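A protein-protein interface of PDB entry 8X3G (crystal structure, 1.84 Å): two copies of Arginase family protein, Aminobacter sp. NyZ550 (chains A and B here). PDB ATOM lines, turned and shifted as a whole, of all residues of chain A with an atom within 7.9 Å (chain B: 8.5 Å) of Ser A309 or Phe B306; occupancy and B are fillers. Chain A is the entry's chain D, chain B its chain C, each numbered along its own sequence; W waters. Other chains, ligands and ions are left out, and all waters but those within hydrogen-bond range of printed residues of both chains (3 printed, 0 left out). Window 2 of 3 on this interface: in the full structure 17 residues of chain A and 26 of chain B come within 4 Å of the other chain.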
ATOM      1  N   ILE A  77     -33.102  -8.795  20.426  1.00  0.00           N
ATOM      2  CA  ILE A  77     -31.915  -8.128  19.909  1.00  0.00           C
ATOM      3  C   ILE A  77     -32.285  -7.257  18.719  1.00  0.00           C
ATOM      4  O   ILE A  77     -31.751  -6.152  18.570  1.00  0.00           O
ATOM      5  CB  ILE A  77     -30.827  -9.168  19.547  1.00  0.00           C
ATOM      6  CG1 ILE A  77     -30.145  -9.615  20.834  1.00  0.00           C
ATOM      7  CG2 ILE A  77     -29.731  -8.524  18.681  1.00  0.00           C
ATOM      8  CD1 ILE A  77     -29.350  -8.539  21.483  1.00  0.00           C
ATOM      9  N   GLU A  80     -33.263  -3.397  18.942  1.00  0.00           N
ATOM     10  CA  GLU A  80     -32.325  -2.302  19.165  1.00  0.00           C
ATOM     11  C   GLU A  80     -31.926  -1.601  17.867  1.00  0.00           C
ATOM     12  O   GLU A  80     -31.192  -0.610  17.907  1.00  0.00           O
ATOM     13  CB  GLU A  80     -31.057  -2.866  19.823  1.00  0.00           C
ATOM     14  CG  GLU A  80     -31.326  -3.671  21.065  1.00  0.00           C
ATOM     15  CD  GLU A  80     -30.079  -4.336  21.550  1.00  0.00           C
ATOM     16  OE1 GLU A  80     -29.014  -4.082  20.929  1.00  0.00           O
ATOM     17  OE2 GLU A  80     -30.162  -5.088  22.552  1.00  0.00           O
ATOM     18  N   PRO A 266     -19.947 -16.374  19.916  1.00  0.00           N
ATOM     19  CA  PRO A 266     -19.767 -17.198  21.134  1.00  0.00           C
ATOM     20  C   PRO A 266     -21.049 -17.915  21.542  1.00  0.00           C
ATOM     21  O   PRO A 266     -20.988 -19.085  21.924  1.00  0.00           O
ATOM     22  CB  PRO A 266     -19.338 -16.179  22.201  1.00  0.00           C
ATOM     23  CG  PRO A 266     -19.932 -14.816  21.673  1.00  0.00           C
ATOM     24  CD  PRO A 266     -19.865 -14.922  20.156  1.00  0.00           C
ATOM     25  N   GLY A 267     -22.199 -17.222  21.515  1.00  0.00           N
ATOM     26  CA  GLY A 267     -23.470 -17.770  21.986  1.00  0.00           C
ATOM     27  C   GLY A 267     -24.145 -18.648  20.936  1.00  0.00           C
ATOM     28  O   GLY A 267     -25.214 -18.285  20.409  1.00  0.00           O
ATOM     29  N   PRO A 304     -28.271 -18.639  23.754  1.00  0.00           N
ATOM     30  CA  PRO A 304     -28.004 -17.411  24.525  1.00  0.00           C
ATOM     31  C   PRO A 304     -27.265 -17.604  25.833  1.00  0.00           C
ATOM     32  O   PRO A 304     -26.582 -16.648  26.258  1.00  0.00           O
ATOM     33  CB  PRO A 304     -29.386 -16.792  24.722  1.00  0.00           C
ATOM     34  CG  PRO A 304     -30.236 -17.407  23.595  1.00  0.00           C
ATOM     35  CD  PRO A 304     -29.563 -18.549  23.015  1.00  0.00           C
ATOM     36  N   PHE A 306     -24.688 -19.115  26.403  1.00  0.00           N
ATOM     37  CA  PHE A 306     -23.246 -19.028  26.166  1.00  0.00           C
ATOM     38  C   PHE A 306     -22.800 -17.732  25.507  1.00  0.00           C
ATOM     39  O   PHE A 306     -21.634 -17.631  25.107  1.00  0.00           O
ATOM     40  CB  PHE A 306     -22.792 -20.156  25.260  1.00  0.00           C
ATOM     41  CG  PHE A 306     -22.780 -21.524  25.890  1.00  0.00           C
ATOM     42  CD1 PHE A 306     -22.487 -21.714  27.220  1.00  0.00           C
ATOM     43  CD2 PHE A 306     -23.022 -22.631  25.069  1.00  0.00           C
ATOM     44  CE1 PHE A 306     -22.449 -23.035  27.787  1.00  0.00           C
ATOM     45  CE2 PHE A 306     -22.966 -23.955  25.608  1.00  0.00           C
ATOM     46  CZ  PHE A 306     -22.713 -24.131  26.981  1.00  0.00           C
ATOM     47  N   ASP A 307     -23.684 -16.760  25.318  1.00  0.00           N
ATOM     48  CA  ASP A 307     -23.284 -15.596  24.525  1.00  0.00           C
ATOM     49  C   ASP A 307     -22.446 -14.636  25.387  1.00  0.00           C
ATOM     50  O   ASP A 307     -22.499 -14.648  26.615  1.00  0.00           O
ATOM     51  CB  ASP A 307     -24.547 -14.875  23.952  1.00  0.00           C
ATOM     52  CG  ASP A 307     -24.327 -14.283  22.563  1.00  0.00           C
ATOM     53  OD1 ASP A 307     -23.170 -14.280  22.081  1.00  0.00           O
ATOM     54  OD2 ASP A 307     -25.352 -13.898  21.933  1.00  0.00           O
ATOM     55  N   ILE A 308     -21.697 -13.760  24.719  1.00  0.00           N
ATOM     56  CA  ILE A 308     -20.943 -12.704  25.396  1.00  0.00           C
ATOM     57  C   ILE A 308     -21.660 -11.410  25.042  1.00  0.00           C
ATOM     58  O   ILE A 308     -21.590 -10.945  23.894  1.00  0.00           O
ATOM     59  CB  ILE A 308     -19.485 -12.688  24.892  1.00  0.00           C
ATOM     60  CG1 ILE A 308     -18.826 -14.004  25.269  1.00  0.00           C
ATOM     61  CG2 ILE A 308     -18.762 -11.448  25.389  1.00  0.00           C
ATOM     62  CD1 ILE A 308     -17.270 -14.191  24.902  1.00  0.00           C
ATOM     63  N   SER A 309     -22.369 -10.853  26.005  1.00  0.00           N
ATOM     64  CA  SER A 309     -23.091  -9.593  25.778  1.00  0.00           C
ATOM     65  C   SER A 309     -23.913  -9.578  24.480  1.00  0.00           C
ATOM     66  O   SER A 309     -23.932  -8.576  23.749  1.00  0.00           O
ATOM     67  CB  SER A 309     -22.103  -8.426  25.810  1.00  0.00           C
ATOM     68  OG  SER A 309     -22.826  -7.274  26.107  1.00  0.00           O
ATOM     69  N   GLY A 310     -24.552 -10.698  24.150  1.00  0.00           N
ATOM     70  CA  GLY A 310     -25.395 -10.783  22.960  1.00  0.00           C
ATOM     71  C   GLY A 310     -24.679 -10.758  21.609  1.00  0.00           C
ATOM     72  O   GLY A 310     -25.337 -10.689  20.559  1.00  0.00           O
ATOM     73  N   THR A 311     -23.356 -10.965  21.577  1.00  0.00           N
ATOM     74  CA  THR A 311     -22.617 -10.804  20.314  1.00  0.00           C
ATOM     75  C   THR A 311     -23.100 -11.744  19.219  1.00  0.00           C
ATOM     76  O   THR A 311     -23.264 -11.314  18.059  1.00  0.00           O
ATOM     77  CB  THR A 311     -21.119 -10.998  20.537  1.00  0.00           C
ATOM     78  OG1 THR A 311     -20.668  -9.852  21.259  1.00  0.00           O
ATOM     79  CG2 THR A 311     -20.406 -10.966  19.190  1.00  0.00           C
ATOM     80  N   ALA A 312     -23.279 -13.049  19.529  1.00  0.00           N
ATOM     81  CA  ALA A 312     -23.716 -13.977  18.488  1.00  0.00           C
ATOM     82  C   ALA A 312     -25.114 -13.625  17.974  1.00  0.00           C
ATOM     83  O   ALA A 312     -25.377 -13.717  16.766  1.00  0.00           O
ATOM     84  CB  ALA A 312     -23.708 -15.453  18.968  1.00  0.00           C
ATOM     85  N   ALA A 313     -26.028 -13.276  18.887  1.00  0.00           N
ATOM     86  CA  ALA A 313     -27.383 -12.911  18.483  1.00  0.00           C
ATOM     87  C   ALA A 313     -27.365 -11.651  17.628  1.00  0.00           C
ATOM     88  O   ALA A 313     -28.122 -11.538  16.659  1.00  0.00           O
ATOM     89  CB  ALA A 313     -28.242 -12.690  19.725  1.00  0.00           C
ATOM     90  N   ARG A 314     -26.531 -10.673  17.988  1.00  0.00           N
ATOM     91  CA  ARG A 314     -26.431  -9.461  17.173  1.00  0.00           C
ATOM     92  C   ARG A 314     -25.846  -9.767  15.812  1.00  0.00           C
ATOM     93  O   ARG A 314     -26.219  -9.140  14.793  1.00  0.00           O
ATOM     94  CB  ARG A 314     -25.513  -8.417  17.874  1.00  0.00           C
ATOM     95  CG  ARG A 314     -26.078  -7.740  19.081  1.00  0.00           C
ATOM     96  CD  ARG A 314     -24.907  -7.076  19.916  1.00  0.00           C
ATOM     97  NE  ARG A 314     -25.293  -6.946  21.313  1.00  0.00           N
ATOM     98  CZ  ARG A 314     -26.285  -6.161  21.648  1.00  0.00           C
ATOM     99  NH1 ARG A 314     -26.933  -5.475  20.727  1.00  0.00           N
ATOM    100  NH2 ARG A 314     -26.658  -6.085  22.922  1.00  0.00           N
ATOM    101  N   GLY B  63     -30.240   5.352  25.613  1.00  0.00           N
ATOM    102  CA  GLY B  63     -30.088   3.925  25.291  1.00  0.00           C
ATOM    103  C   GLY B  63     -29.866   3.059  26.513  1.00  0.00           C
ATOM    104  O   GLY B  63     -30.463   3.335  27.557  1.00  0.00           O
ATOM    105  N   LYS B  64     -29.048   2.021  26.355  1.00  0.00           N
ATOM    106  CA  LYS B  64     -28.758   1.090  27.474  1.00  0.00           C
ATOM    107  C   LYS B  64     -27.929   1.818  28.528  1.00  0.00           C
ATOM    108  O   LYS B  64     -27.006   2.546  28.165  1.00  0.00           O
ATOM    109  CB  LYS B  64     -28.029  -0.158  26.978  1.00  0.00           C
ATOM    110  CG  LYS B  64     -28.875  -1.079  26.108  1.00  0.00           C
ATOM    111  CD  LYS B  64     -28.119  -2.274  25.566  1.00  0.00           C
ATOM    112  CE  LYS B  64     -27.949  -2.243  24.063  1.00  0.00           C
ATOM    113  NZ  LYS B  64     -26.670  -2.857  23.643  1.00  0.00           N
ATOM    114  N   PRO B  65     -28.244   1.639  29.816  1.00  0.00           N
ATOM    115  CA  PRO B  65     -27.547   2.353  30.859  1.00  0.00           C
ATOM    116  C   PRO B  65     -26.254   1.637  31.261  1.00  0.00           C
ATOM    117  O   PRO B  65     -26.125   0.471  30.981  1.00  0.00           O
ATOM    118  CB  PRO B  65     -28.554   2.307  32.012  1.00  0.00           C
ATOM    119  CG  PRO B  65     -29.803   1.655  31.455  1.00  0.00           C
ATOM    120  CD  PRO B  65     -29.318   0.793  30.315  1.00  0.00           C
ATOM    121  N   GLY B  66     -25.334   2.371  31.880  1.00  0.00           N
ATOM    122  CA  GLY B  66     -24.095   1.737  32.371  1.00  0.00           C
ATOM    123  C   GLY B  66     -22.874   2.622  32.273  1.00  0.00           C
ATOM    124  O   GLY B  66     -21.913   2.339  32.993  1.00  0.00           O
ATOM    125  N   SER B  67     -22.924   3.679  31.463  1.00  0.00           N
ATOM    126  CA  SER B  67     -21.703   4.496  31.218  1.00  0.00           C
ATOM    127  C   SER B  67     -21.215   5.228  32.480  1.00  0.00           C
ATOM    128  O   SER B  67     -20.045   5.595  32.527  1.00  0.00           O
ATOM    129  CB  SER B  67     -21.919   5.441  30.060  1.00  0.00           C
ATOM    130  OG  SER B  67     -22.668   6.575  30.448  1.00  0.00           O
ATOM    131  N   SER B 262     -17.845  -5.848  17.453  1.00  0.00           N
ATOM    132  CA  SER B 262     -18.413  -6.131  18.779  1.00  0.00           C
ATOM    133  C   SER B 262     -17.551  -7.102  19.591  1.00  0.00           C
ATOM    134  O   SER B 262     -17.445  -6.959  20.814  1.00  0.00           O
ATOM    135  CB  SER B 262     -19.830  -6.660  18.627  1.00  0.00           C
ATOM    136  OG  SER B 262     -20.520  -5.771  17.773  1.00  0.00           O
ATOM    137  N   ALA B 265     -15.026  -5.164  21.557  1.00  0.00           N
ATOM    138  CA  ALA B 265     -15.543  -4.131  22.486  1.00  0.00           C
ATOM    139  C   ALA B 265     -17.016  -4.409  22.823  1.00  0.00           C
ATOM    140  O   ALA B 265     -17.877  -3.663  22.387  1.00  0.00           O
ATOM    141  CB  ALA B 265     -15.325  -2.774  21.882  1.00  0.00           C
ATOM    142  N   PRO B 266     -17.303  -5.486  23.579  1.00  0.00           N
ATOM    143  CA  PRO B 266     -18.669  -5.828  23.939  1.00  0.00           C
ATOM    144  C   PRO B 266     -19.243  -4.866  24.990  1.00  0.00           C
ATOM    145  O   PRO B 266     -20.403  -4.606  24.950  1.00  0.00           O
ATOM    146  CB  PRO B 266     -18.548  -7.225  24.558  1.00  0.00           C
ATOM    147  CG  PRO B 266     -17.126  -7.302  25.062  1.00  0.00           C
ATOM    148  CD  PRO B 266     -16.328  -6.438  24.110  1.00  0.00           C
ATOM    149  N   GLY B 267     -18.389  -4.362  25.878  1.00  0.00           N
ATOM    150  CA  GLY B 267     -18.932  -3.533  26.968  1.00  0.00           C
ATOM    151  C   GLY B 267     -19.063  -2.090  26.545  1.00  0.00           C
ATOM    152  O   GLY B 267     -18.315  -1.211  27.031  1.00  0.00           O
ATOM    153  N   VAL B 268     -19.995  -1.824  25.617  1.00  0.00           N
ATOM    154  CA  VAL B 268     -20.293  -0.472  25.145  1.00  0.00           C
ATOM    155  C   VAL B 268     -21.820  -0.362  25.101  1.00  0.00           C
ATOM    156  O   VAL B 268     -22.530  -1.375  25.114  1.00  0.00           O
ATOM    157  CB  VAL B 268     -19.703  -0.164  23.750  1.00  0.00           C
ATOM    158  CG1 VAL B 268     -18.122  -0.253  23.718  1.00  0.00           C
ATOM    159  CG2 VAL B 268     -20.238  -1.185  22.717  1.00  0.00           C
ATOM    160  N   THR B 269     -22.315   0.904  25.052  1.00  0.00           N
ATOM    161  CA  THR B 269     -23.747   1.171  25.182  1.00  0.00           C
ATOM    162  C   THR B 269     -24.549   0.587  24.020  1.00  0.00           C
ATOM    163  O   THR B 269     -25.690   0.138  24.194  1.00  0.00           O
ATOM    164  CB  THR B 269     -23.920   2.730  25.310  1.00  0.00           C
ATOM    165  OG1 THR B 269     -23.501   3.019  26.653  1.00  0.00           O
ATOM    166  CG2 THR B 269     -25.362   3.063  25.300  1.00  0.00           C
ATOM    167  N   SER B 270     -24.013   0.632  22.813  1.00  0.00           N
ATOM    168  CA  SER B 270     -24.755   0.058  21.679  1.00  0.00           C
ATOM    169  C   SER B 270     -23.745  -0.468  20.650  1.00  0.00           C
ATOM    170  O   SER B 270     -22.785   0.220  20.333  1.00  0.00           O
ATOM    171  CB  SER B 270     -25.706   1.112  21.068  1.00  0.00           C
ATOM    172  OG  SER B 270     -24.909   2.082  20.442  1.00  0.00           O
ATOM    173  N   THR B 271     -23.949  -1.663  20.123  1.00  0.00           N
ATOM    174  CA  THR B 271     -22.939  -2.166  19.193  1.00  0.00           C
ATOM    175  C   THR B 271     -23.605  -3.031  18.143  1.00  0.00           C
ATOM    176  O   THR B 271     -24.735  -3.508  18.311  1.00  0.00           O
ATOM    177  CB  THR B 271     -21.840  -2.975  19.873  1.00  0.00           C
ATOM    178  OG1 THR B 271     -20.815  -3.235  18.880  1.00  0.00           O
ATOM    179  CG2 THR B 271     -22.480  -4.269  20.404  1.00  0.00           C
ATOM    180  N   PRO B 273     -22.009  -5.887  15.133  1.00  0.00           N
ATOM    181  CA  PRO B 273     -20.766  -6.443  14.587  1.00  0.00           C
ATOM    182  C   PRO B 273     -20.490  -5.879  13.190  1.00  0.00           C
ATOM    183  O   PRO B 273     -21.398  -5.484  12.475  1.00  0.00           O
ATOM    184  CB  PRO B 273     -21.033  -7.974  14.598  1.00  0.00           C
ATOM    185  CG  PRO B 273     -22.348  -8.133  14.951  1.00  0.00           C
ATOM    186  CD  PRO B 273     -22.842  -6.946  15.718  1.00  0.00           C
ATOM    187  N   GLU B 301     -19.450   6.275  26.381  1.00  0.00           N
ATOM    188  CA  GLU B 301     -20.308   5.109  26.009  1.00  0.00           C
ATOM    189  C   GLU B 301     -19.703   3.726  26.340  1.00  0.00           C
ATOM    190  O   GLU B 301     -20.231   2.745  25.826  1.00  0.00           O
ATOM    191  CB  GLU B 301     -20.834   5.263  24.583  1.00  0.00           C
ATOM    192  CG  GLU B 301     -21.611   6.554  24.379  1.00  0.00           C
ATOM    193  CD  GLU B 301     -22.892   6.711  25.183  1.00  0.00           C
ATOM    194  OE1 GLU B 301     -23.284   5.757  25.868  1.00  0.00           O
ATOM    195  OE2 GLU B 301     -23.495   7.791  25.118  1.00  0.00           O
ATOM    196  N   LEU B 302     -18.644   3.661  27.136  1.00  0.00           N
ATOM    197  CA  LEU B 302     -18.191   2.342  27.634  1.00  0.00           C
ATOM    198  C   LEU B 302     -19.283   1.894  28.615  1.00  0.00           C
ATOM    199  O   LEU B 302     -19.869   2.764  29.264  1.00  0.00           O
ATOM    200  CB  LEU B 302     -16.843   2.484  28.330  1.00  0.00           C
ATOM    201  CG  LEU B 302     -15.619   2.513  27.420  1.00  0.00           C
ATOM    202  CD1 LEU B 302     -14.358   2.739  28.237  1.00  0.00           C
ATOM    203  CD2 LEU B 302     -15.516   1.224  26.621  1.00  0.00           C
ATOM    204  N   CYS B 303     -19.556   0.601  28.705  1.00  0.00           N
ATOM    205  CA  CYS B 303     -20.674   0.121  29.555  1.00  0.00           C
ATOM    206  C   CYS B 303     -20.190  -1.117  30.307  1.00  0.00           C
ATOM    207  O   CYS B 303     -20.378  -2.216  29.805  1.00  0.00           O
ATOM    208  CB  CYS B 303     -21.908  -0.135  28.702  1.00  0.00           C
ATOM    209  SG  CYS B 303     -23.390  -0.543  29.650  1.00  0.00           S
ATOM    210  N   PRO B 304     -19.541  -0.943  31.469  1.00  0.00           N
ATOM    211  CA  PRO B 304     -18.923  -2.070  32.174  1.00  0.00           C
ATOM    212  C   PRO B 304     -19.900  -3.219  32.485  1.00  0.00           C
ATOM    213  O   PRO B 304     -19.482  -4.342  32.415  1.00  0.00           O
ATOM    214  CB  PRO B 304     -18.373  -1.420  33.449  1.00  0.00           C
ATOM    215  CG  PRO B 304     -18.173   0.028  33.075  1.00  0.00           C
ATOM    216  CD  PRO B 304     -19.316   0.338  32.133  1.00  0.00           C
ATOM    217  N   ILE B 305     -21.141  -2.908  32.846  1.00  0.00           N
ATOM    218  CA  ILE B 305     -22.053  -4.021  33.188  1.00  0.00           C
ATOM    219  C   ILE B 305     -22.219  -5.019  32.016  1.00  0.00           C
ATOM    220  O   ILE B 305     -22.541  -6.198  32.238  1.00  0.00           O
ATOM    221  CB  ILE B 305     -23.419  -3.467  33.675  1.00  0.00           C
ATOM    222  CG1 ILE B 305     -24.221  -4.550  34.391  1.00  0.00           C
ATOM    223  CG2 ILE B 305     -24.291  -2.985  32.553  1.00  0.00           C
ATOM    224  CD1 ILE B 305     -25.092  -3.981  35.465  1.00  0.00           C
ATOM    225  N   PHE B 306     -21.984  -4.587  30.770  1.00  0.00           N
ATOM    226  CA  PHE B 306     -22.059  -5.472  29.605  1.00  0.00           C
ATOM    227  C   PHE B 306     -20.694  -5.995  29.197  1.00  0.00           C
ATOM    228  O   PHE B 306     -20.578  -6.631  28.150  1.00  0.00           O
ATOM    229  CB  PHE B 306     -22.660  -4.743  28.386  1.00  0.00           C
ATOM    230  CG  PHE B 306     -24.131  -4.413  28.514  1.00  0.00           C
ATOM    231  CD1 PHE B 306     -24.932  -5.057  29.446  1.00  0.00           C
ATOM    232  CD2 PHE B 306     -24.669  -3.360  27.774  1.00  0.00           C
ATOM    233  CE1 PHE B 306     -26.283  -4.736  29.575  1.00  0.00           C
ATOM    234  CE2 PHE B 306     -26.021  -3.020  27.900  1.00  0.00           C
ATOM    235  CZ  PHE B 306     -26.817  -3.708  28.816  1.00  0.00           C
ATOM    236  N   ASP B 307     -19.654  -5.676  29.944  1.00  0.00           N
ATOM    237  CA  ASP B 307     -18.319  -6.050  29.498  1.00  0.00           C
ATOM    238  C   ASP B 307     -18.110  -7.477  30.009  1.00  0.00           C
ATOM    239  O   ASP B 307     -18.735  -7.922  30.984  1.00  0.00           O
ATOM    240  CB  ASP B 307     -17.301  -5.020  30.007  1.00  0.00           C
ATOM    241  CG  ASP B 307     -16.174  -4.669  28.964  1.00  0.00           C
ATOM    242  OD1 ASP B 307     -16.214  -5.241  27.817  1.00  0.00           O
ATOM    243  OD2 ASP B 307     -15.239  -3.848  29.353  1.00  0.00           O
ATOM    244  N   ILE B 308     -17.300  -8.232  29.294  1.00  0.00           N
ATOM    245  CA  ILE B 308     -16.901  -9.562  29.736  1.00  0.00           C
ATOM    246  C   ILE B 308     -15.388  -9.541  29.822  1.00  0.00           C
ATOM    247  O   ILE B 308     -14.724  -9.087  28.883  1.00  0.00           O
ATOM    248  CB  ILE B 308     -17.400 -10.666  28.811  1.00  0.00           C
ATOM    249  CG1 ILE B 308     -18.780 -11.143  29.310  1.00  0.00           C
ATOM    250  CG2 ILE B 308     -16.431 -11.955  28.854  1.00  0.00           C
ATOM    251  CD1 ILE B 308     -19.878 -10.134  29.057  1.00  0.00           C
ATOM    252  N   SER B 309     -14.870  -9.931  30.978  1.00  0.00           N
ATOM    253  CA  SER B 309     -13.447  -9.959  31.250  1.00  0.00           C
ATOM    254  C   SER B 309     -12.848  -8.598  30.953  1.00  0.00           C
ATOM    255  O   SER B 309     -11.661  -8.462  30.614  1.00  0.00           O
ATOM    256  CB  SER B 309     -12.788 -11.101  30.453  1.00  0.00           C
ATOM    257  OG  SER B 309     -11.407 -11.252  30.710  1.00  0.00           O
ATOM    258  N   GLY B 310     -13.676  -7.543  31.096  1.00  0.00           N
ATOM    259  CA  GLY B 310     -13.125  -6.210  30.901  1.00  0.00           C
ATOM    260  C   GLY B 310     -12.668  -5.913  29.483  1.00  0.00           C
ATOM    261  O   GLY B 310     -11.861  -5.002  29.291  1.00  0.00           O
ATOM    262  N   THR B 311     -13.189  -6.630  28.471  1.00  0.00           N
ATOM    263  CA  THR B 311     -12.605  -6.533  27.112  1.00  0.00           C
ATOM    264  C   THR B 311     -12.658  -5.111  26.519  1.00  0.00           C
ATOM    265  O   THR B 311     -11.629  -4.581  26.064  1.00  0.00           O
ATOM    266  CB  THR B 311     -13.323  -7.546  26.195  1.00  0.00           C
ATOM    267  OG1 THR B 311     -13.053  -8.868  26.696  1.00  0.00           O
ATOM    268  CG2 THR B 311     -12.833  -7.400  24.731  1.00  0.00           C
ATOM    269  N   ALA B 312     -13.825  -4.456  26.509  1.00  0.00           N
ATOM    270  CA  ALA B 312     -13.892  -3.126  25.904  1.00  0.00           C
ATOM    271  C   ALA B 312     -13.026  -2.126  26.662  1.00  0.00           C
ATOM    272  O   ALA B 312     -12.401  -1.241  26.052  1.00  0.00           O
ATOM    273  CB  ALA B 312     -15.312  -2.596  25.886  1.00  0.00           C
HETATM  274  O   HOH W   1     -27.194  -2.103  19.497  1.00  0.00           O
HETATM  275  O   HOH W   2     -18.437  -9.945  22.266  1.00  0.00           O
HETATM  276  O   HOH W   3     -22.599  -5.490  23.696  1.00  0.00           O
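Among the printed residues, merely in contact across the chains: Ile A308 with Ile B308, Ser A309 with Pro B266, Arg A314 with Thr B271 and Arg A314 with Pro B273.
The side-chain amino group (NZ) of Lys B64 lies within salt-bridge range of the side-chain carboxylate (OE1) of Glu A80 (3.8 Å).
The backbone carbonyl oxygen of Phe B306 sits at hydrogen-bond distance from the side-chain hydroxyl of Ser A309 (3.1 Å).
NH2 of Arg A314 lies close to NZ of Lys B64, 3.3 Å away.
The backbone carbonyl oxygen (O) of Thr B269 is in hydrogen-bond range of the side-chain amino group (NZ) of Lys B64 (3.2 Å).
OG of Ser B262 lies within hydrogen-bond range of OG1 of Thr B271 (2.8 Å).
O of Ile B308 is in hydrogen-bond range of OG1 of Thr B311, 2.8 Å away.
The side-chain carboxylate of Glu A80 is in salt-bridge range of the guanidinium group of Arg A314.
O of Ile A308 lies within hydrogen-bond range of OG1 of Thr A311 (3.0 Å).
NE of Arg A314 sits at hydrogen-bond distance from O of Ser A309, at 3.2 Å.
Water W2 bridges OG1 of Thr A311 (2.4 Å) and O of Ser B262 (3.5 Å).
Water W3 lies within hydrogen-bond range of the backbone carbonyl oxygen (O) of Pro B266 and the side-chain hydroxyl (OG) of Ser A309.
Water W1 lies within hydrogen-bond range of the side-chain carboxylate of Glu A80 (3.0 Å) and the backbone carbonyl oxygen of Thr B271 (3.1 Å).
Of the 26 printed residues of chain B, 6 touch a printed residue of chain A.
Printed residues of chain B that touch a printed residue of chain A: Lys B64, Pro B266, Thr B271, Pro B273, Phe B306 and Ile B308.
Hydrophobic or aromatic side chains of chain B within 4 Å of the printed part of chain A: Pro B266, Pro B273, Phe B306 and Ile B308.
Hydrophobic or aromatic side chains of chain A within 4 Å of the printed part of chain B: Ile A308.
Among the printed residues, 7 pairs touch across the chains.
Among the printed residues, Asp or Glu carboxylates within 4 Å of a Lys or Arg side-chain nitrogen of the other chain: Glu A80 with Lys B64.
Ile A308 touches its own counterpart, Ile B308.
Ser A309 touches Pro B266, but with the chains exchanged Pro A266 does not touch Ser B309 (11.7 Å).
Ser A309 touches Phe B306, but with the chains exchanged Phe A306 does not touch Ser B309 (11.8 Å).
10 positions are printed for both chains.
Of the 7 pairs that touch across the chains among the printed residues, 1 has its exchanged pair printed and touching as well.
Of the printed residues of chain B, Ile A308 touches Ile B308 (3.8 Å).
Of the printed residues of chain B, Ser A309 touches Pro B266 (3.8 Å) and Phe B306 (3.1 Å).
Thr A311 touches none of the printed residues of chain B.
Of the printed residues of chain B, Arg A314 touches Lys B64 (3.3 Å), Thr B271 (3.7 Å) and Pro B273 (3.7 Å).
Printed residues of chain A within 4 Å of Pro B273: Arg A314 (3.7 Å).
Of chain A, only Ser A309 (3.1 Å) comes within 4 Å of Phe B306.
Of the printed residues of chain A, Ile B308 touches Ile A308.
Ser B309 touches none of the printed residues of chain A.
The nearest printed residue of chain B that does not touch Ser A309 is Ile B308 (4.005 Å).
The nearest printed residue of chain B that does not touch Ile A308 is Pro B266 (4.3 Å).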
